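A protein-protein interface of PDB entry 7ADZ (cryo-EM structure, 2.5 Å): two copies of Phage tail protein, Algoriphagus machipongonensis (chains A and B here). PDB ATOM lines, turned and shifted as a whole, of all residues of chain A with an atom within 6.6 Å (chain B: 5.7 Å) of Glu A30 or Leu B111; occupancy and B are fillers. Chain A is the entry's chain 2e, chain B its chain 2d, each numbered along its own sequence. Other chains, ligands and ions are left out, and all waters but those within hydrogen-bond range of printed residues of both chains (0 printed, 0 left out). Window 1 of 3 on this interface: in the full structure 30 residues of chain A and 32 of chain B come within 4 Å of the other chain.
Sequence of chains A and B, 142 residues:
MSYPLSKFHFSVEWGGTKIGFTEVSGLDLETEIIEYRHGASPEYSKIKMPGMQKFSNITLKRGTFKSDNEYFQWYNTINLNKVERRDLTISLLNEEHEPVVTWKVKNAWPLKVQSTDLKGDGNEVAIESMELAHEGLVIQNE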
ATOM      1  N   ASP A  28      23.468  14.673 -20.643  1.00  0.00           N
ATOM      2  CA  ASP A  28      22.122  14.560 -21.223  1.00  0.00           C
ATOM      3  C   ASP A  28      21.017  14.145 -20.245  1.00  0.00           C
ATOM      4  O   ASP A  28      21.282  13.488 -19.239  1.00  0.00           O
ATOM      5  CB  ASP A  28      22.143  13.523 -22.336  1.00  0.00           C
ATOM      6  CG  ASP A  28      23.070  13.855 -23.489  1.00  0.00           C
ATOM      7  OD1 ASP A  28      23.126  14.982 -23.908  1.00  0.00           O
ATOM      8  OD2 ASP A  28      23.730  12.949 -23.948  1.00  0.00           O
ATOM      9  N   LEU A  29      19.768  14.491 -20.584  1.00  0.00           N
ATOM     10  CA  LEU A  29      18.553  14.097 -19.851  1.00  0.00           C
ATOM     11  C   LEU A  29      17.542  13.493 -20.837  1.00  0.00           C
ATOM     12  O   LEU A  29      17.342  14.062 -21.907  1.00  0.00           O
ATOM     13  CB  LEU A  29      17.911  15.337 -19.216  1.00  0.00           C
ATOM     14  CG  LEU A  29      18.749  16.141 -18.203  1.00  0.00           C
ATOM     15  CD1 LEU A  29      18.052  17.429 -17.892  1.00  0.00           C
ATOM     16  CD2 LEU A  29      18.923  15.370 -16.946  1.00  0.00           C
ATOM     17  N   GLU A  30      16.863  12.393 -20.484  1.00  0.00           N
ATOM     18  CA  GLU A  30      15.885  11.790 -21.407  1.00  0.00           C
ATOM     19  C   GLU A  30      14.698  11.080 -20.746  1.00  0.00           C
ATOM     20  O   GLU A  30      14.828  10.520 -19.660  1.00  0.00           O
ATOM     21  CB  GLU A  30      16.605  10.796 -22.317  1.00  0.00           C
ATOM     22  CG  GLU A  30      15.727  10.114 -23.347  1.00  0.00           C
ATOM     23  CD  GLU A  30      16.477   9.231 -24.250  1.00  0.00           C
ATOM     24  OE1 GLU A  30      17.668   9.338 -24.313  1.00  0.00           O
ATOM     25  OE2 GLU A  30      15.854   8.386 -24.856  1.00  0.00           O
ATOM     26  N   THR A  31      13.521  11.129 -21.390  1.00  0.00           N
ATOM     27  CA  THR A  31      12.361  10.378 -20.902  1.00  0.00           C
ATOM     28  C   THR A  31      11.716   9.530 -21.985  1.00  0.00           C
ATOM     29  O   THR A  31      11.822   9.824 -23.173  1.00  0.00           O
ATOM     30  CB  THR A  31      11.263  11.293 -20.356  1.00  0.00           C
ATOM     31  OG1 THR A  31      10.743  12.102 -21.409  1.00  0.00           O
ATOM     32  CG2 THR A  31      11.823  12.151 -19.322  1.00  0.00           C
ATOM     33  N   GLU A  32      10.978   8.520 -21.542  1.00  0.00           N
ATOM     34  CA  GLU A  32      10.197   7.630 -22.396  1.00  0.00           C
ATOM     35  C   GLU A  32       8.829   8.220 -22.751  1.00  0.00           C
ATOM     36  O   GLU A  32       8.336   9.126 -22.068  1.00  0.00           O
ATOM     37  CB  GLU A  32      10.000   6.289 -21.705  1.00  0.00           C
ATOM     38  CG  GLU A  32      11.266   5.492 -21.393  1.00  0.00           C
ATOM     39  CD  GLU A  32      11.991   4.951 -22.603  1.00  0.00           C
ATOM     40  OE1 GLU A  32      11.585   5.227 -23.699  1.00  0.00           O
ATOM     41  OE2 GLU A  32      12.948   4.207 -22.423  1.00  0.00           O
ATOM     42  N   ILE A  33       8.218   7.714 -23.820  1.00  0.00           N
ATOM     43  CA  ILE A  33       6.873   8.125 -24.228  1.00  0.00           C
ATOM     44  C   ILE A  33       5.874   6.977 -24.209  1.00  0.00           C
ATOM     45  O   ILE A  33       6.130   5.915 -24.771  1.00  0.00           O
ATOM     46  CB  ILE A  33       6.867   8.725 -25.655  1.00  0.00           C
ATOM     47  CG1 ILE A  33       7.757   9.956 -25.683  1.00  0.00           C
ATOM     48  CG2 ILE A  33       5.407   9.073 -26.097  1.00  0.00           C
ATOM     49  CD1 ILE A  33       8.034  10.498 -27.060  1.00  0.00           C
ATOM     50  N   MET A  52       9.055   6.827 -17.830  1.00  0.00           N
ATOM     51  CA  MET A  52      10.195   6.788 -16.915  1.00  0.00           C
ATOM     52  C   MET A  52      11.409   7.588 -17.420  1.00  0.00           C
ATOM     53  O   MET A  52      11.526   7.889 -18.611  1.00  0.00           O
ATOM     54  CB  MET A  52      10.564   5.345 -16.635  1.00  0.00           C
ATOM     55  CG  MET A  52       9.484   4.606 -15.845  1.00  0.00           C
ATOM     56  SD  MET A  52       9.848   2.883 -15.512  1.00  0.00           S
ATOM     57  CE  MET A  52      11.098   3.001 -14.246  1.00  0.00           C
ATOM     58  N   GLN A  53      12.298   7.959 -16.489  1.00  0.00           N
ATOM     59  CA  GLN A  53      13.490   8.777 -16.773  1.00  0.00           C
ATOM     60  C   GLN A  53      14.753   7.952 -17.049  1.00  0.00           C
ATOM     61  O   GLN A  53      14.923   6.869 -16.490  1.00  0.00           O
ATOM     62  CB  GLN A  53      13.825   9.614 -15.540  1.00  0.00           C
ATOM     63  CG  GLN A  53      12.717  10.476 -14.955  1.00  0.00           C
ATOM     64  CD  GLN A  53      12.243  11.607 -15.762  1.00  0.00           C
ATOM     65  OE1 GLN A  53      13.031  12.448 -16.187  1.00  0.00           O
ATOM     66  NE2 GLN A  53      10.941  11.668 -15.953  1.00  0.00           N
ATOM     67  N   LYS A  54      15.665   8.510 -17.851  1.00  0.00           N
ATOM     68  CA  LYS A  54      16.987   7.947 -18.145  1.00  0.00           C
ATOM     69  C   LYS A  54      18.110   8.978 -18.082  1.00  0.00           C
ATOM     70  O   LYS A  54      17.901  10.178 -18.300  1.00  0.00           O
ATOM     71  CB  LYS A  54      17.013   7.314 -19.523  1.00  0.00           C
ATOM     72  CG  LYS A  54      16.127   6.140 -19.677  1.00  0.00           C
ATOM     73  CD  LYS A  54      16.187   5.562 -21.072  1.00  0.00           C
ATOM     74  CE  LYS A  54      15.457   6.456 -22.070  1.00  0.00           C
ATOM     75  NZ  LYS A  54      15.185   5.767 -23.344  1.00  0.00           N
ATOM     76  N   PHE A  55      19.326   8.492 -17.833  1.00  0.00           N
ATOM     77  CA  PHE A  55      20.520   9.330 -17.874  1.00  0.00           C
ATOM     78  C   PHE A  55      21.620   8.669 -18.694  1.00  0.00           C
ATOM     79  O   PHE A  55      21.723   7.445 -18.711  1.00  0.00           O
ATOM     80  CB  PHE A  55      21.043   9.593 -16.475  1.00  0.00           C
ATOM     81  CG  PHE A  55      20.075  10.291 -15.611  1.00  0.00           C
ATOM     82  CD1 PHE A  55      19.305   9.583 -14.720  1.00  0.00           C
ATOM     83  CD2 PHE A  55      19.889  11.646 -15.711  1.00  0.00           C
ATOM     84  CE1 PHE A  55      18.375  10.208 -13.953  1.00  0.00           C
ATOM     85  CE2 PHE A  55      18.954  12.269 -14.937  1.00  0.00           C
ATOM     86  CZ  PHE A  55      18.196  11.550 -14.063  1.00  0.00           C
ATOM     87  N   SER A  56      22.459   9.471 -19.339  1.00  0.00           N
ATOM     88  CA  SER A  56      23.618   8.968 -20.088  1.00  0.00           C
ATOM     89  C   SER A  56      24.869   8.903 -19.217  1.00  0.00           C
ATOM     90  O   SER A  56      24.974   9.634 -18.226  1.00  0.00           O
ATOM     91  CB  SER A  56      23.911   9.853 -21.283  1.00  0.00           C
ATOM     92  OG  SER A  56      22.870   9.830 -22.214  1.00  0.00           O
ATOM     93  N   ASN B  57       9.191  14.047 -34.395  1.00  0.00           N
ATOM     94  CA  ASN B  57       9.545  14.965 -33.310  1.00  0.00           C
ATOM     95  C   ASN B  57      10.234  16.199 -33.877  1.00  0.00           C
ATOM     96  O   ASN B  57      10.881  16.127 -34.918  1.00  0.00           O
ATOM     97  CB  ASN B  57      10.440  14.313 -32.281  1.00  0.00           C
ATOM     98  CG  ASN B  57       9.779  13.219 -31.528  1.00  0.00           C
ATOM     99  OD1 ASN B  57       8.552  13.120 -31.418  1.00  0.00           O
ATOM    100  ND2 ASN B  57      10.585  12.372 -30.990  1.00  0.00           N
ATOM    101  N   TYR B  75      11.453  21.407 -18.913  1.00  0.00           N
ATOM    102  CA  TYR B  75      11.660  19.971 -18.753  1.00  0.00           C
ATOM    103  C   TYR B  75      11.298  19.535 -17.339  1.00  0.00           C
ATOM    104  O   TYR B  75      10.646  18.517 -17.112  1.00  0.00           O
ATOM    105  CB  TYR B  75      13.095  19.591 -19.061  1.00  0.00           C
ATOM    106  CG  TYR B  75      13.331  18.119 -19.066  1.00  0.00           C
ATOM    107  CD1 TYR B  75      13.022  17.407 -20.198  1.00  0.00           C
ATOM    108  CD2 TYR B  75      13.830  17.477 -17.966  1.00  0.00           C
ATOM    109  CE1 TYR B  75      13.208  16.074 -20.248  1.00  0.00           C
ATOM    110  CE2 TYR B  75      14.017  16.123 -18.012  1.00  0.00           C
ATOM    111  CZ  TYR B  75      13.705  15.425 -19.153  1.00  0.00           C
ATOM    112  OH  TYR B  75      13.886  14.075 -19.211  1.00  0.00           O
ATOM    113  N   TRP B 109       5.585  18.943 -25.811  1.00  0.00           N
ATOM    114  CA  TRP B 109       6.290  18.753 -24.543  1.00  0.00           C
ATOM    115  C   TRP B 109       7.666  18.124 -24.817  1.00  0.00           C
ATOM    116  O   TRP B 109       7.800  17.286 -25.669  1.00  0.00           O
ATOM    117  CB  TRP B 109       5.460  18.008 -23.453  1.00  0.00           C
ATOM    118  CG  TRP B 109       4.951  16.656 -23.812  1.00  0.00           C
ATOM    119  CD1 TRP B 109       3.808  16.373 -24.458  1.00  0.00           C
ATOM    120  CD2 TRP B 109       5.581  15.402 -23.547  1.00  0.00           C
ATOM    121  NE1 TRP B 109       3.671  15.035 -24.615  1.00  0.00           N
ATOM    122  CE2 TRP B 109       4.752  14.406 -24.073  1.00  0.00           C
ATOM    123  CE3 TRP B 109       6.771  15.026 -22.922  1.00  0.00           C
ATOM    124  CZ2 TRP B 109       5.058  13.060 -23.988  1.00  0.00           C
ATOM    125  CZ3 TRP B 109       7.076  13.700 -22.849  1.00  0.00           C
ATOM    126  CH2 TRP B 109       6.225  12.728 -23.379  1.00  0.00           C
ATOM    127  N   PRO B 110       8.689  18.520 -24.058  1.00  0.00           N
ATOM    128  CA  PRO B 110      10.109  18.137 -24.047  1.00  0.00           C
ATOM    129  C   PRO B 110      10.409  16.687 -23.699  1.00  0.00           C
ATOM    130  O   PRO B 110      10.233  16.270 -22.559  1.00  0.00           O
ATOM    131  CB  PRO B 110      10.666  19.026 -22.938  1.00  0.00           C
ATOM    132  CG  PRO B 110       9.749  20.144 -22.842  1.00  0.00           C
ATOM    133  CD  PRO B 110       8.394  19.589 -23.135  1.00  0.00           C
ATOM    134  N   LEU B 111      10.883  15.938 -24.678  1.00  0.00           N
ATOM    135  CA  LEU B 111      11.310  14.564 -24.470  1.00  0.00           C
ATOM    136  C   LEU B 111      12.707  14.511 -23.926  1.00  0.00           C
ATOM    137  O   LEU B 111      13.049  13.698 -23.072  1.00  0.00           O
ATOM    138  CB  LEU B 111      11.325  13.793 -25.779  1.00  0.00           C
ATOM    139  CG  LEU B 111      10.036  13.559 -26.437  1.00  0.00           C
ATOM    140  CD1 LEU B 111      10.319  12.977 -27.773  1.00  0.00           C
ATOM    141  CD2 LEU B 111       9.171  12.612 -25.595  1.00  0.00           C
ATOM    142  N   LYS B 112      13.535  15.357 -24.511  1.00  0.00           N
ATOM    143  CA  LYS B 112      14.953  15.357 -24.240  1.00  0.00           C
ATOM    144  C   LYS B 112      15.604  16.724 -24.289  1.00  0.00           C
ATOM    145  O   LYS B 112      15.318  17.539 -25.168  1.00  0.00           O
ATOM    146  CB  LYS B 112      15.613  14.426 -25.254  1.00  0.00           C
ATOM    147  CG  LYS B 112      17.080  14.221 -25.113  1.00  0.00           C
ATOM    148  CD  LYS B 112      17.555  13.198 -26.122  1.00  0.00           C
ATOM    149  CE  LYS B 112      19.057  12.969 -26.023  1.00  0.00           C
ATOM    150  NZ  LYS B 112      19.528  11.964 -27.016  1.00  0.00           N
ATOM    151  N   VAL B 113      16.520  16.958 -23.357  1.00  0.00           N
ATOM    152  CA  VAL B 113      17.327  18.170 -23.336  1.00  0.00           C
ATOM    153  C   VAL B 113      18.794  17.771 -23.337  1.00  0.00           C
ATOM    154  O   VAL B 113      19.238  17.004 -22.488  1.00  0.00           O
ATOM    155  CB  VAL B 113      16.989  19.057 -22.119  1.00  0.00           C
ATOM    156  CG1 VAL B 113      17.871  20.301 -22.107  1.00  0.00           C
ATOM    157  CG2 VAL B 113      15.532  19.474 -22.193  1.00  0.00           C
ATOM    158  N   GLU B 131      14.426  18.367 -27.905  1.00  0.00           N
ATOM    159  CA  GLU B 131      13.556  17.563 -28.772  1.00  0.00           C
ATOM    160  C   GLU B 131      12.134  17.480 -28.213  1.00  0.00           C
ATOM    161  O   GLU B 131      11.918  17.076 -27.058  1.00  0.00           O
ATOM    162  CB  GLU B 131      14.150  16.175 -28.969  1.00  0.00           C
ATOM    163  CG  GLU B 131      13.365  15.257 -29.877  1.00  0.00           C
ATOM    164  CD  GLU B 131      14.073  13.939 -30.077  1.00  0.00           C
ATOM    165  OE1 GLU B 131      15.206  13.854 -29.670  1.00  0.00           O
ATOM    166  OE2 GLU B 131      13.493  13.008 -30.607  1.00  0.00           O
ATOM    167  N   LEU B 132      11.164  17.879 -29.043  1.00  0.00           N
ATOM    168  CA  LEU B 132       9.755  17.925 -28.655  1.00  0.00           C
ATOM    169  C   LEU B 132       8.792  16.933 -29.308  1.00  0.00           C
ATOM    170  O   LEU B 132       8.738  16.767 -30.530  1.00  0.00           O
ATOM    171  CB  LEU B 132       9.193  19.313 -29.008  1.00  0.00           C
ATOM    172  CG  LEU B 132       9.837  20.557 -28.369  1.00  0.00           C
ATOM    173  CD1 LEU B 132       9.250  21.781 -28.975  1.00  0.00           C
ATOM    174  CD2 LEU B 132       9.575  20.571 -26.908  1.00  0.00           C
ATOM    175  N   ALA B 133       7.942  16.356 -28.473  1.00  0.00           N
ATOM    176  CA  ALA B 133       6.845  15.490 -28.880  1.00  0.00           C
ATOM    177  C   ALA B 133       5.643  16.375 -29.132  1.00  0.00           C
ATOM    178  O   ALA B 133       5.528  17.423 -28.502  1.00  0.00           O
ATOM    179  CB  ALA B 133       6.536  14.467 -27.813  1.00  0.00           C
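O of Val B113 lies within hydrogen-bond range of N of Leu A29 (3.2 Å). The backbone carbonyl oxygen (O) of Leu B111 sits at hydrogen-bond distance from the backbone NH (N) of Thr A31, at 3.1 Å.
The backbone carbonyl oxygen of Lys B112 is in hydrogen-bond range of the backbone NH of Glu B131 (3.0 Å). The side-chain amino group (NZ) of Lys A54 lies within salt-bridge range of the side-chain carboxylate (OE2) of Glu A30 (3.1 Å). The backbone carbonyl oxygen of Trp B109 is in hydrogen-bond range of the backbone NH of Ala B133, at 3.0 Å. The backbone carbonyl oxygen (O) of Glu B131 is in hydrogen-bond range of the backbone NH (N) of Leu B111 (2.8 Å).
Asp A28 touches Val B113. Leu A29 touches Lys B112. Glu A30 touches Tyr B75. O of Leu B111 touches CA of Glu A30, 3.8 Å away. OH of Tyr B75 touches CG2 of Thr A31, 2.8 Å away. Trp B109 touches Ile A33 (CH2 to CG1, 3.9 Å). CD2 of Leu B111 touches CD1 of Ile A33, at 2.8 Å. Tyr B75 touches Gln A53.
Of the printed residues of chain B, Asp A28 touches Val B113 (3.99 Å). Of the printed residues of chain B, Leu A29 touches Lys B112 and Val B113. Of chain B, only Tyr B75 (3.5 Å) and Leu B111 (3.8 Å) come within 4 Å of Glu A30. Of the printed residues of chain A, Trp B109 touches Ile A33. Leu B111 touches three residues of chain A. The nearest residue of chain A that does not touch Leu B111 is Leu A29 (4.5 Å). The nearest printed residue of chain B that does not touch Leu A29 is Tyr B75 (4.04 Å).
Hydrophobic or aromatic side chains of chain A within 4 Å of the printed part of chain B: Leu A29 and Ile A33. Hydrophobic or aromatic side chains of chain B that line the printed part of chain A: Tyr B75, Trp B109 and Leu B111. Among the printed residues, 10 pairs touch across the chains. Among the printed residues, no Asp or Glu carboxylate lies within 4 Å of a Lys or Arg side-chain nitrogen of the other chain.
No position is printed for both chains. Of the 10 pairs that touch across the chains among the printed residues, none has its exchanged pair printed and touching as well.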
